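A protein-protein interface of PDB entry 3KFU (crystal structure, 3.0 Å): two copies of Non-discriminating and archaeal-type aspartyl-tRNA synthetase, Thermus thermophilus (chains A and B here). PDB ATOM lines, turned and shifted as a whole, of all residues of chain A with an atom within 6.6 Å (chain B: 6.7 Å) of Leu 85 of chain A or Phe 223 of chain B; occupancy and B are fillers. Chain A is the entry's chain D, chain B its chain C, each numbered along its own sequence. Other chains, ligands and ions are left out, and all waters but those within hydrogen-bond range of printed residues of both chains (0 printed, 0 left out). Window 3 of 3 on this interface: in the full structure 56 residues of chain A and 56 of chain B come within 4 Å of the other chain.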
ATOM      1  N   ARG A   2     -31.465  13.844 -14.879  1.00  0.00           N
ATOM      2  CA  ARG A   2     -31.288  13.227 -16.186  1.00  0.00           C
ATOM      3  C   ARG A   2     -31.150  11.712 -16.091  1.00  0.00           C
ATOM      4  O   ARG A   2     -30.566  11.186 -15.144  1.00  0.00           O
ATOM      5  CB  ARG A   2     -30.062  13.815 -16.888  1.00  0.00           C
ATOM      6  CG  ARG A   2     -29.757  13.189 -18.240  1.00  0.00           C
ATOM      7  CD  ARG A   2     -28.374  13.585 -18.723  1.00  0.00           C
ATOM      8  NE  ARG A   2     -28.053  13.013 -20.027  1.00  0.00           N
ATOM      9  CZ  ARG A   2     -26.873  13.144 -20.622  1.00  0.00           C
ATOM     10  NH1 ARG A   2     -25.902  13.822 -20.025  1.00  0.00           N
ATOM     11  NH2 ARG A   2     -26.660  12.596 -21.809  1.00  0.00           N
ATOM     12  N   LEU A  18     -34.318  13.157 -21.040  1.00  0.00           N
ATOM     13  CA  LEU A  18     -33.182  12.712 -21.836  1.00  0.00           C
ATOM     14  C   LEU A  18     -32.365  13.878 -22.382  1.00  0.00           C
ATOM     15  O   LEU A  18     -32.912  14.922 -22.737  1.00  0.00           O
ATOM     16  CB  LEU A  18     -33.657  11.841 -22.998  1.00  0.00           C
ATOM     17  CG  LEU A  18     -34.348  10.534 -22.628  1.00  0.00           C
ATOM     18  CD1 LEU A  18     -34.738   9.778 -23.884  1.00  0.00           C
ATOM     19  CD2 LEU A  18     -33.436   9.694 -21.760  1.00  0.00           C
ATOM     20  N   LEU A  19     -31.053  13.687 -22.445  1.00  0.00           N
ATOM     21  CA  LEU A  19     -30.166  14.653 -23.077  1.00  0.00           C
ATOM     22  C   LEU A  19     -29.279  13.945 -24.087  1.00  0.00           C
ATOM     23  O   LEU A  19     -28.558  13.009 -23.741  1.00  0.00           O
ATOM     24  CB  LEU A  19     -29.306  15.361 -22.032  1.00  0.00           C
ATOM     25  CG  LEU A  19     -30.034  16.324 -21.094  1.00  0.00           C
ATOM     26  CD1 LEU A  19     -29.077  16.873 -20.053  1.00  0.00           C
ATOM     27  CD2 LEU A  19     -30.678  17.453 -21.882  1.00  0.00           C
ATOM     28  N   GLY A  20     -29.337  14.386 -25.339  1.00  0.00           N
ATOM     29  CA  GLY A  20     -28.514  13.794 -26.376  1.00  0.00           C
ATOM     30  C   GLY A  20     -28.631  14.494 -27.714  1.00  0.00           C
ATOM     31  O   GLY A  20     -28.987  15.667 -27.787  1.00  0.00           O
ATOM     32  N   PHE A  21     -28.323  13.763 -28.779  1.00  0.00           N
ATOM     33  CA  PHE A  21     -28.394  14.306 -30.127  1.00  0.00           C
ATOM     34  C   PHE A  21     -29.476  13.606 -30.929  1.00  0.00           C
ATOM     35  O   PHE A  21     -29.815  12.454 -30.658  1.00  0.00           O
ATOM     36  CB  PHE A  21     -27.047  14.152 -30.836  1.00  0.00           C
ATOM     37  CG  PHE A  21     -25.914  14.835 -30.133  1.00  0.00           C
ATOM     38  CD1 PHE A  21     -25.222  14.192 -29.123  1.00  0.00           C
ATOM     39  CD2 PHE A  21     -25.541  16.120 -30.481  1.00  0.00           C
ATOM     40  CE1 PHE A  21     -24.181  14.818 -28.472  1.00  0.00           C
ATOM     41  CE2 PHE A  21     -24.502  16.750 -29.833  1.00  0.00           C
ATOM     42  CZ  PHE A  21     -23.819  16.096 -28.827  1.00  0.00           C
ATOM     43  N   ARG A  37     -29.432   9.722 -29.518  1.00  0.00           N
ATOM     44  CA  ARG A  37     -28.154   9.164 -29.107  1.00  0.00           C
ATOM     45  C   ARG A  37     -27.543   9.951 -27.951  1.00  0.00           C
ATOM     46  O   ARG A  37     -27.511  11.179 -27.973  1.00  0.00           O
ATOM     47  CB  ARG A  37     -27.177   9.140 -30.283  1.00  0.00           C
ATOM     48  CG  ARG A  37     -25.856   8.462 -29.969  1.00  0.00           C
ATOM     49  CD  ARG A  37     -24.829   8.699 -31.065  1.00  0.00           C
ATOM     50  NE  ARG A  37     -24.365  10.084 -31.089  1.00  0.00           N
ATOM     51  CZ  ARG A  37     -24.680  10.967 -32.031  1.00  0.00           C
ATOM     52  NH1 ARG A  37     -25.458  10.616 -33.046  1.00  0.00           N
ATOM     53  NH2 ARG A  37     -24.209  12.201 -31.961  1.00  0.00           N
ATOM     54  N   SER A  57     -28.759  17.535 -34.118  1.00  0.00           N
ATOM     55  CA  SER A  57     -29.075  18.648 -33.232  1.00  0.00           C
ATOM     56  C   SER A  57     -29.133  18.187 -31.776  1.00  0.00           C
ATOM     57  O   SER A  57     -29.661  17.115 -31.477  1.00  0.00           O
ATOM     58  CB  SER A  57     -30.413  19.274 -33.627  1.00  0.00           C
ATOM     59  OG  SER A  57     -30.415  19.663 -34.990  1.00  0.00           O
ATOM     60  N   ALA A  58     -28.590  18.998 -30.872  1.00  0.00           N
ATOM     61  CA  ALA A  58     -28.661  18.700 -29.445  1.00  0.00           C
ATOM     62  C   ALA A  58     -30.092  18.865 -28.944  1.00  0.00           C
ATOM     63  O   ALA A  58     -30.747  19.860 -29.245  1.00  0.00           O
ATOM     64  CB  ALA A  58     -27.717  19.596 -28.667  1.00  0.00           C
ATOM     65  N   LEU A  59     -30.570  17.891 -28.177  1.00  0.00           N
ATOM     66  CA  LEU A  59     -31.966  17.874 -27.747  1.00  0.00           C
ATOM     67  C   LEU A  59     -32.164  17.605 -26.256  1.00  0.00           C
ATOM     68  O   LEU A  59     -31.323  16.987 -25.599  1.00  0.00           O
ATOM     69  CB  LEU A  59     -32.751  16.827 -28.536  1.00  0.00           C
ATOM     70  CG  LEU A  59     -33.055  17.103 -30.006  1.00  0.00           C
ATOM     71  CD1 LEU A  59     -33.766  15.906 -30.614  1.00  0.00           C
ATOM     72  CD2 LEU A  59     -33.898  18.360 -30.150  1.00  0.00           C
ATOM     73  N   ARG A  60     -33.296  18.071 -25.740  1.00  0.00           N
ATOM     74  CA  ARG A  60     -33.746  17.734 -24.396  1.00  0.00           C
ATOM     75  C   ARG A  60     -35.159  17.167 -24.488  1.00  0.00           C
ATOM     76  O   ARG A  60     -36.085  17.859 -24.910  1.00  0.00           O
ATOM     77  CB  ARG A  60     -33.732  18.967 -23.493  1.00  0.00           C
ATOM     78  CG  ARG A  60     -34.365  18.743 -22.129  1.00  0.00           C
ATOM     79  CD  ARG A  60     -34.397  20.027 -21.312  1.00  0.00           C
ATOM     80  NE  ARG A  60     -35.125  19.852 -20.059  1.00  0.00           N
ATOM     81  CZ  ARG A  60     -36.440  19.996 -19.932  1.00  0.00           C
ATOM     82  NH1 ARG A  60     -37.181  20.320 -20.983  1.00  0.00           N
ATOM     83  NH2 ARG A  60     -37.018  19.815 -18.751  1.00  0.00           N
ATOM     84  N   GLU A  83     -37.400  19.854 -26.575  1.00  0.00           N
ATOM     85  CA  GLU A  83     -36.693  21.127 -26.593  1.00  0.00           C
ATOM     86  C   GLU A  83     -35.409  21.016 -27.407  1.00  0.00           C
ATOM     87  O   GLU A  83     -34.726  19.994 -27.365  1.00  0.00           O
ATOM     88  CB  GLU A  83     -36.376  21.566 -25.161  1.00  0.00           C
ATOM     89  CG  GLU A  83     -35.570  22.850 -25.055  1.00  0.00           C
ATOM     90  CD  GLU A  83     -35.297  23.246 -23.616  1.00  0.00           C
ATOM     91  OE1 GLU A  83     -34.543  24.218 -23.396  1.00  0.00           O
ATOM     92  OE2 GLU A  83     -35.838  22.585 -22.704  1.00  0.00           O
ATOM     93  N   VAL A  84     -35.086  22.071 -28.147  1.00  0.00           N
ATOM     94  CA  VAL A  84     -33.883  22.079 -28.972  1.00  0.00           C
ATOM     95  C   VAL A  84     -32.810  22.979 -28.362  1.00  0.00           C
ATOM     96  O   VAL A  84     -32.977  24.195 -28.279  1.00  0.00           O
ATOM     97  CB  VAL A  84     -34.190  22.538 -30.409  1.00  0.00           C
ATOM     98  CG1 VAL A  84     -32.983  22.311 -31.307  1.00  0.00           C
ATOM     99  CG2 VAL A  84     -35.401  21.799 -30.947  1.00  0.00           C
ATOM    100  N   LEU A  85     -31.709  22.369 -27.934  1.00  0.00           N
ATOM    101  CA  LEU A  85     -30.636  23.101 -27.270  1.00  0.00           C
ATOM    102  C   LEU A  85     -29.670  23.720 -28.275  1.00  0.00           C
ATOM    103  O   LEU A  85     -29.022  24.725 -27.989  1.00  0.00           O
ATOM    104  CB  LEU A  85     -29.872  22.177 -26.321  1.00  0.00           C
ATOM    105  CG  LEU A  85     -30.725  21.295 -25.413  1.00  0.00           C
ATOM    106  CD1 LEU A  85     -29.845  20.382 -24.571  1.00  0.00           C
ATOM    107  CD2 LEU A  85     -31.622  22.149 -24.537  1.00  0.00           C
ATOM    108  N   SER A  86     -29.575  23.110 -29.452  1.00  0.00           N
ATOM    109  CA  SER A  86     -28.670  23.593 -30.486  1.00  0.00           C
ATOM    110  C   SER A  86     -28.960  22.931 -31.825  1.00  0.00           C
ATOM    111  O   SER A  86     -28.623  21.766 -32.033  1.00  0.00           O
ATOM    112  CB  SER A  86     -27.220  23.336 -30.089  1.00  0.00           C
ATOM    113  OG  SER A  86     -26.336  23.918 -31.026  1.00  0.00           O
ATOM    114  N   PRO A  87     -29.581  23.684 -32.741  1.00  0.00           N
ATOM    115  CA  PRO A  87     -30.002  23.193 -34.056  1.00  0.00           C
ATOM    116  C   PRO A  87     -28.827  22.991 -34.997  1.00  0.00           C
ATOM    117  O   PRO A  87     -27.881  23.777 -34.982  1.00  0.00           O
ATOM    118  CB  PRO A  87     -30.878  24.331 -34.595  1.00  0.00           C
ATOM    119  CG  PRO A  87     -31.156  25.220 -33.421  1.00  0.00           C
ATOM    120  CD  PRO A  87     -29.966  25.087 -32.534  1.00  0.00           C
ATOM    121  N   VAL B 187     -16.523  16.481 -27.515  1.00  0.00           N
ATOM    122  CA  VAL B 187     -17.673  16.677 -26.644  1.00  0.00           C
ATOM    123  C   VAL B 187     -18.956  16.252 -27.351  1.00  0.00           C
ATOM    124  O   VAL B 187     -19.893  15.765 -26.718  1.00  0.00           O
ATOM    125  CB  VAL B 187     -17.795  18.139 -26.186  1.00  0.00           C
ATOM    126  CG1 VAL B 187     -19.109  18.361 -25.459  1.00  0.00           C
ATOM    127  CG2 VAL B 187     -16.625  18.509 -25.299  1.00  0.00           C
ATOM    128  N   GLU B 191     -19.572  13.615 -24.839  1.00  0.00           N
ATOM    129  CA  GLU B 191     -20.256  14.533 -23.925  1.00  0.00           C
ATOM    130  C   GLU B 191     -19.360  15.064 -22.809  1.00  0.00           C
ATOM    131  O   GLU B 191     -19.411  16.247 -22.486  1.00  0.00           O
ATOM    132  CB  GLU B 191     -21.498  13.878 -23.315  1.00  0.00           C
ATOM    133  CG  GLU B 191     -22.567  13.492 -24.318  1.00  0.00           C
ATOM    134  CD  GLU B 191     -23.759  12.827 -23.661  1.00  0.00           C
ATOM    135  OE1 GLU B 191     -23.887  12.928 -22.422  1.00  0.00           O
ATOM    136  OE2 GLU B 191     -24.564  12.200 -24.379  1.00  0.00           O
ATOM    137  N   ARG B 192     -18.562  14.182 -22.211  1.00  0.00           N
ATOM    138  CA  ARG B 192     -17.676  14.555 -21.113  1.00  0.00           C
ATOM    139  C   ARG B 192     -16.329  13.883 -21.304  1.00  0.00           C
ATOM    140  O   ARG B 192     -16.233  12.660 -21.280  1.00  0.00           O
ATOM    141  CB  ARG B 192     -18.261  14.117 -19.772  1.00  0.00           C
ATOM    142  CG  ARG B 192     -19.738  14.400 -19.615  1.00  0.00           C
ATOM    143  CD  ARG B 192     -20.383  13.437 -18.630  1.00  0.00           C
ATOM    144  NE  ARG B 192     -20.278  13.894 -17.250  1.00  0.00           N
ATOM    145  CZ  ARG B 192     -21.091  14.791 -16.704  1.00  0.00           C
ATOM    146  NH1 ARG B 192     -22.061  15.337 -17.424  1.00  0.00           N
ATOM    147  NH2 ARG B 192     -20.931  15.151 -15.439  1.00  0.00           N
ATOM    148  N   MET B 221     -16.764  19.391 -20.768  1.00  0.00           N
ATOM    149  CA  MET B 221     -18.048  18.702 -20.669  1.00  0.00           C
ATOM    150  C   MET B 221     -19.186  19.429 -21.379  1.00  0.00           C
ATOM    151  O   MET B 221     -19.185  20.655 -21.484  1.00  0.00           O
ATOM    152  CB  MET B 221     -18.414  18.442 -19.206  1.00  0.00           C
ATOM    153  CG  MET B 221     -18.604  19.691 -18.375  1.00  0.00           C
ATOM    154  SD  MET B 221     -18.990  19.307 -16.657  1.00  0.00           S
ATOM    155  CE  MET B 221     -20.479  18.330 -16.859  1.00  0.00           C
ATOM    156  N   GLY B 222     -20.160  18.657 -21.854  1.00  0.00           N
ATOM    157  CA  GLY B 222     -21.273  19.198 -22.615  1.00  0.00           C
ATOM    158  C   GLY B 222     -22.591  19.203 -21.863  1.00  0.00           C
ATOM    159  O   GLY B 222     -22.680  18.711 -20.738  1.00  0.00           O
ATOM    160  N   PHE B 223     -23.618  19.762 -22.494  1.00  0.00           N
ATOM    161  CA  PHE B 223     -24.939  19.883 -21.884  1.00  0.00           C
ATOM    162  C   PHE B 223     -24.869  20.485 -20.484  1.00  0.00           C
ATOM    163  O   PHE B 223     -25.434  19.946 -19.532  1.00  0.00           O
ATOM    164  CB  PHE B 223     -25.656  18.531 -21.857  1.00  0.00           C
ATOM    165  CG  PHE B 223     -25.888  17.946 -23.218  1.00  0.00           C
ATOM    166  CD1 PHE B 223     -26.926  18.403 -24.014  1.00  0.00           C
ATOM    167  CD2 PHE B 223     -25.065  16.945 -23.705  1.00  0.00           C
ATOM    168  CE1 PHE B 223     -27.137  17.872 -25.269  1.00  0.00           C
ATOM    169  CE2 PHE B 223     -25.271  16.409 -24.961  1.00  0.00           C
ATOM    170  CZ  PHE B 223     -26.307  16.872 -25.744  1.00  0.00           C
ATOM    171  N   ILE B 224     -24.166  21.604 -20.367  1.00  0.00           N
ATOM    172  CA  ILE B 224     -24.106  22.346 -19.117  1.00  0.00           C
ATOM    173  C   ILE B 224     -25.156  23.451 -19.129  1.00  0.00           C
ATOM    174  O   ILE B 224     -25.838  23.662 -20.133  1.00  0.00           O
ATOM    175  CB  ILE B 224     -22.720  22.985 -18.909  1.00  0.00           C
ATOM    176  CG1 ILE B 224     -22.486  24.100 -19.933  1.00  0.00           C
ATOM    177  CG2 ILE B 224     -21.632  21.932 -19.008  1.00  0.00           C
ATOM    178  CD1 ILE B 224     -21.157  24.804 -19.783  1.00  0.00           C
ATOM    179  N   ALA B 225     -25.279  24.157 -18.012  1.00  0.00           N
ATOM    180  CA  ALA B 225     -26.190  25.289 -17.925  1.00  0.00           C
ATOM    181  C   ALA B 225     -25.428  26.590 -18.150  1.00  0.00           C
ATOM    182  O   ALA B 225     -25.814  27.419 -18.974  1.00  0.00           O
ATOM    183  CB  ALA B 225     -26.884  25.304 -16.573  1.00  0.00           C
ATOM    184  N   ASP B 229     -21.617  25.370 -13.651  1.00  0.00           N
ATOM    185  CA  ASP B 229     -21.477  23.919 -13.674  1.00  0.00           C
ATOM    186  C   ASP B 229     -20.004  23.536 -13.621  1.00  0.00           C
ATOM    187  O   ASP B 229     -19.615  22.591 -12.931  1.00  0.00           O
ATOM    188  CB  ASP B 229     -22.113  23.337 -14.940  1.00  0.00           C
ATOM    189  CG  ASP B 229     -23.605  23.599 -15.022  1.00  0.00           C
ATOM    190  OD1 ASP B 229     -24.086  24.566 -14.393  1.00  0.00           O
ATOM    191  OD2 ASP B 229     -24.297  22.837 -15.731  1.00  0.00           O
ATOM    192  N   HIS B 354     -21.175  28.011 -28.885  1.00  0.00           N
ATOM    193  CA  HIS B 354     -21.531  26.776 -29.578  1.00  0.00           C
ATOM    194  C   HIS B 354     -22.389  26.987 -30.822  1.00  0.00           C
ATOM    195  O   HIS B 354     -22.568  26.063 -31.613  1.00  0.00           O
ATOM    196  CB  HIS B 354     -22.215  25.802 -28.621  1.00  0.00           C
ATOM    197  CG  HIS B 354     -23.479  26.328 -28.015  1.00  0.00           C
ATOM    198  ND1 HIS B 354     -24.716  26.151 -28.598  1.00  0.00           N
ATOM    199  CD2 HIS B 354     -23.701  27.014 -26.870  1.00  0.00           C
ATOM    200  CE1 HIS B 354     -25.642  26.708 -27.841  1.00  0.00           C
ATOM    201  NE2 HIS B 354     -25.052  27.240 -26.784  1.00  0.00           N
ATOM    202  N   ARG B 355     -22.920  28.195 -30.988  1.00  0.00           N
ATOM    203  CA  ARG B 355     -23.696  28.543 -32.174  1.00  0.00           C
ATOM    204  C   ARG B 355     -22.764  29.064 -33.265  1.00  0.00           C
ATOM    205  O   ARG B 355     -21.947  29.949 -33.012  1.00  0.00           O
ATOM    206  CB  ARG B 355     -24.741  29.605 -31.836  1.00  0.00           C
ATOM    207  CG  ARG B 355     -25.594  29.284 -30.617  1.00  0.00           C
ATOM    208  CD  ARG B 355     -26.635  28.213 -30.913  1.00  0.00           C
ATOM    209  NE  ARG B 355     -27.756  28.731 -31.694  1.00  0.00           N
ATOM    210  CZ  ARG B 355     -27.864  28.624 -33.014  1.00  0.00           C
ATOM    211  NH1 ARG B 355     -26.917  28.011 -33.713  1.00  0.00           N
ATOM    212  NH2 ARG B 355     -28.920  29.127 -33.637  1.00  0.00           N
ATOM    213  N   MET B 384     -23.871  21.755 -32.118  1.00  0.00           N
ATOM    214  CA  MET B 384     -22.938  21.644 -31.010  1.00  0.00           C
ATOM    215  C   MET B 384     -23.639  22.021 -29.709  1.00  0.00           C
ATOM    216  O   MET B 384     -24.254  23.080 -29.621  1.00  0.00           O
ATOM    217  CB  MET B 384     -21.751  22.572 -31.244  1.00  0.00           C
ATOM    218  CG  MET B 384     -20.537  22.220 -30.427  1.00  0.00           C
ATOM    219  SD  MET B 384     -19.887  20.613 -30.894  1.00  0.00           S
ATOM    220  CE  MET B 384     -18.381  20.603 -29.933  1.00  0.00           C
ATOM    221  N   PRO B 385     -23.544  21.156 -28.690  1.00  0.00           N
ATOM    222  CA  PRO B 385     -24.211  21.389 -27.403  1.00  0.00           C
ATOM    223  C   PRO B 385     -23.573  22.535 -26.636  1.00  0.00           C
ATOM    224  O   PRO B 385     -22.401  22.828 -26.855  1.00  0.00           O
ATOM    225  CB  PRO B 385     -23.960  20.087 -26.635  1.00  0.00           C
ATOM    226  CG  PRO B 385     -23.492  19.104 -27.651  1.00  0.00           C
ATOM    227  CD  PRO B 385     -22.790  19.896 -28.696  1.00  0.00           C
ATOM    228  N   PRO B 386     -24.338  23.182 -25.746  1.00  0.00           N
ATOM    229  CA  PRO B 386     -23.765  24.147 -24.805  1.00  0.00           C
ATOM    230  C   PRO B 386     -22.691  23.467 -23.974  1.00  0.00           C
ATOM    231  O   PRO B 386     -23.003  22.572 -23.192  1.00  0.00           O
ATOM    232  CB  PRO B 386     -24.954  24.509 -23.918  1.00  0.00           C
ATOM    233  CG  PRO B 386     -26.133  24.302 -24.784  1.00  0.00           C
ATOM    234  CD  PRO B 386     -25.803  23.108 -25.633  1.00  0.00           C
ATOM    235  N   HIS B 387     -21.441  23.883 -24.144  1.00  0.00           N
ATOM    236  CA  HIS B 387     -20.325  23.221 -23.486  1.00  0.00           C
ATOM    237  C   HIS B 387     -19.329  24.225 -22.922  1.00  0.00           C
ATOM    238  O   HIS B 387     -19.498  25.435 -23.065  1.00  0.00           O
ATOM    239  CB  HIS B 387     -19.619  22.307 -24.476  1.00  0.00           C
ATOM    240  CG  HIS B 387     -19.086  23.022 -25.676  1.00  0.00           C
ATOM    241  ND1 HIS B 387     -17.838  23.607 -25.698  1.00  0.00           N
ATOM    242  CD2 HIS B 387     -19.633  23.258 -26.891  1.00  0.00           C
ATOM    243  CE1 HIS B 387     -17.637  24.165 -26.877  1.00  0.00           C
ATOM    244  NE2 HIS B 387     -18.712  23.968 -27.621  1.00  0.00           N
ATOM    245  N   GLY B 388     -18.287  23.707 -22.285  1.00  0.00           N
ATOM    246  CA  GLY B 388     -17.259  24.534 -21.683  1.00  0.00           C
ATOM    247  C   GLY B 388     -16.215  23.663 -21.016  1.00  0.00           C
ATOM    248  O   GLY B 388     -16.416  22.461 -20.864  1.00  0.00           O
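No position is printed for both chains. Of the 8 pairs that touch across the chains among the printed residues, none has its exchanged pair printed and touching as well.
The guanidinium group of Arg 2 of chain A is in salt-bridge range of the side-chain carboxylate of Glu 191 of chain B, 2.9 Å away. The backbone carbonyl oxygen (O) of Met 384 of chain B sits at hydrogen-bond distance from the side-chain hydroxyl (OG) of Ser 86 of chain A (2.6 Å).
Gly 20 of chain A touches Phe 223 of chain B. Phe 21 of chain A touches Pro 385 of chain B (CZ to CG, 3.2 Å). Phe 223 of chain B touches Ala 58 of chain A. Leu 85 of chain A touches Phe 223 of chain B (CD1 to CD1, 3.6 Å). His 354 of chain B touches Leu 85 of chain A (CE1 to O, 3.9 Å). Ser 86 of chain A touches His 354 of chain B.
A ring nitrogen (ND1) of His 354 of chain B sits at hydrogen-bond distance from the backbone carbonyl oxygen of Met 384 of chain B, 3.3 Å away. The backbone carbonyl oxygen (O) of Pro 386 of chain B is in hydrogen-bond range of the backbone NH (N) of Phe 223 of chain B, 3.0 Å away. The backbone carbonyl oxygen (O) of Gly 20 of chain A lies within hydrogen-bond range of the backbone NH (N) of Leu 59 of chain A (2.8 Å). N of Gly 222 of chain B is in hydrogen-bond range of O of Glu 191 of chain B. The backbone carbonyl oxygen of Ser 86 of chain A is in hydrogen-bond range of the backbone NH of Ala 58 of chain A (3.0 Å). The backbone NH of Phe 21 of chain A lies within hydrogen-bond range of the backbone carbonyl oxygen of Arg 37 of chain A, at 2.8 Å.
Of the printed residues of chain B, Gly 20 of chain A touches Phe 223. Printed residues of chain B within 4 Å of Ser 86 of chain A: His 354 and Met 384. Printed residues of chain A within 4 Å of Glu 191 of chain B: Arg 2 (2.9 Å). Gly 222 of chain B touches none of the printed residues of chain A. Of the printed residues of chain A, Phe 223 of chain B touches Gly 20 (3.6 Å), Ala 58 (3.9 Å) and Leu 85 (3.6 Å). Ile 224 of chain B touches none of the printed residues of chain A. The nearest residue of chain B that does not touch Leu 85 of chain A is Pro 386 of chain B (4.2 Å). The nearest printed residue of chain A that does not touch Phe 223 of chain B is Phe 21 of chain A (4.01 Å). The nearest printed residue of chain A that does not touch Met 384 of chain B is Ala 58 of chain A (4.9 Å).
Of the 16 printed residues of chain B, 5 touch a printed residue of chain A. Hydrophobic or aromatic side chains of chain A within 4 Å of the printed part of chain B: Phe 21, Ala 58 and Leu 85. Among the printed residues, 8 pairs touch across the chains.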
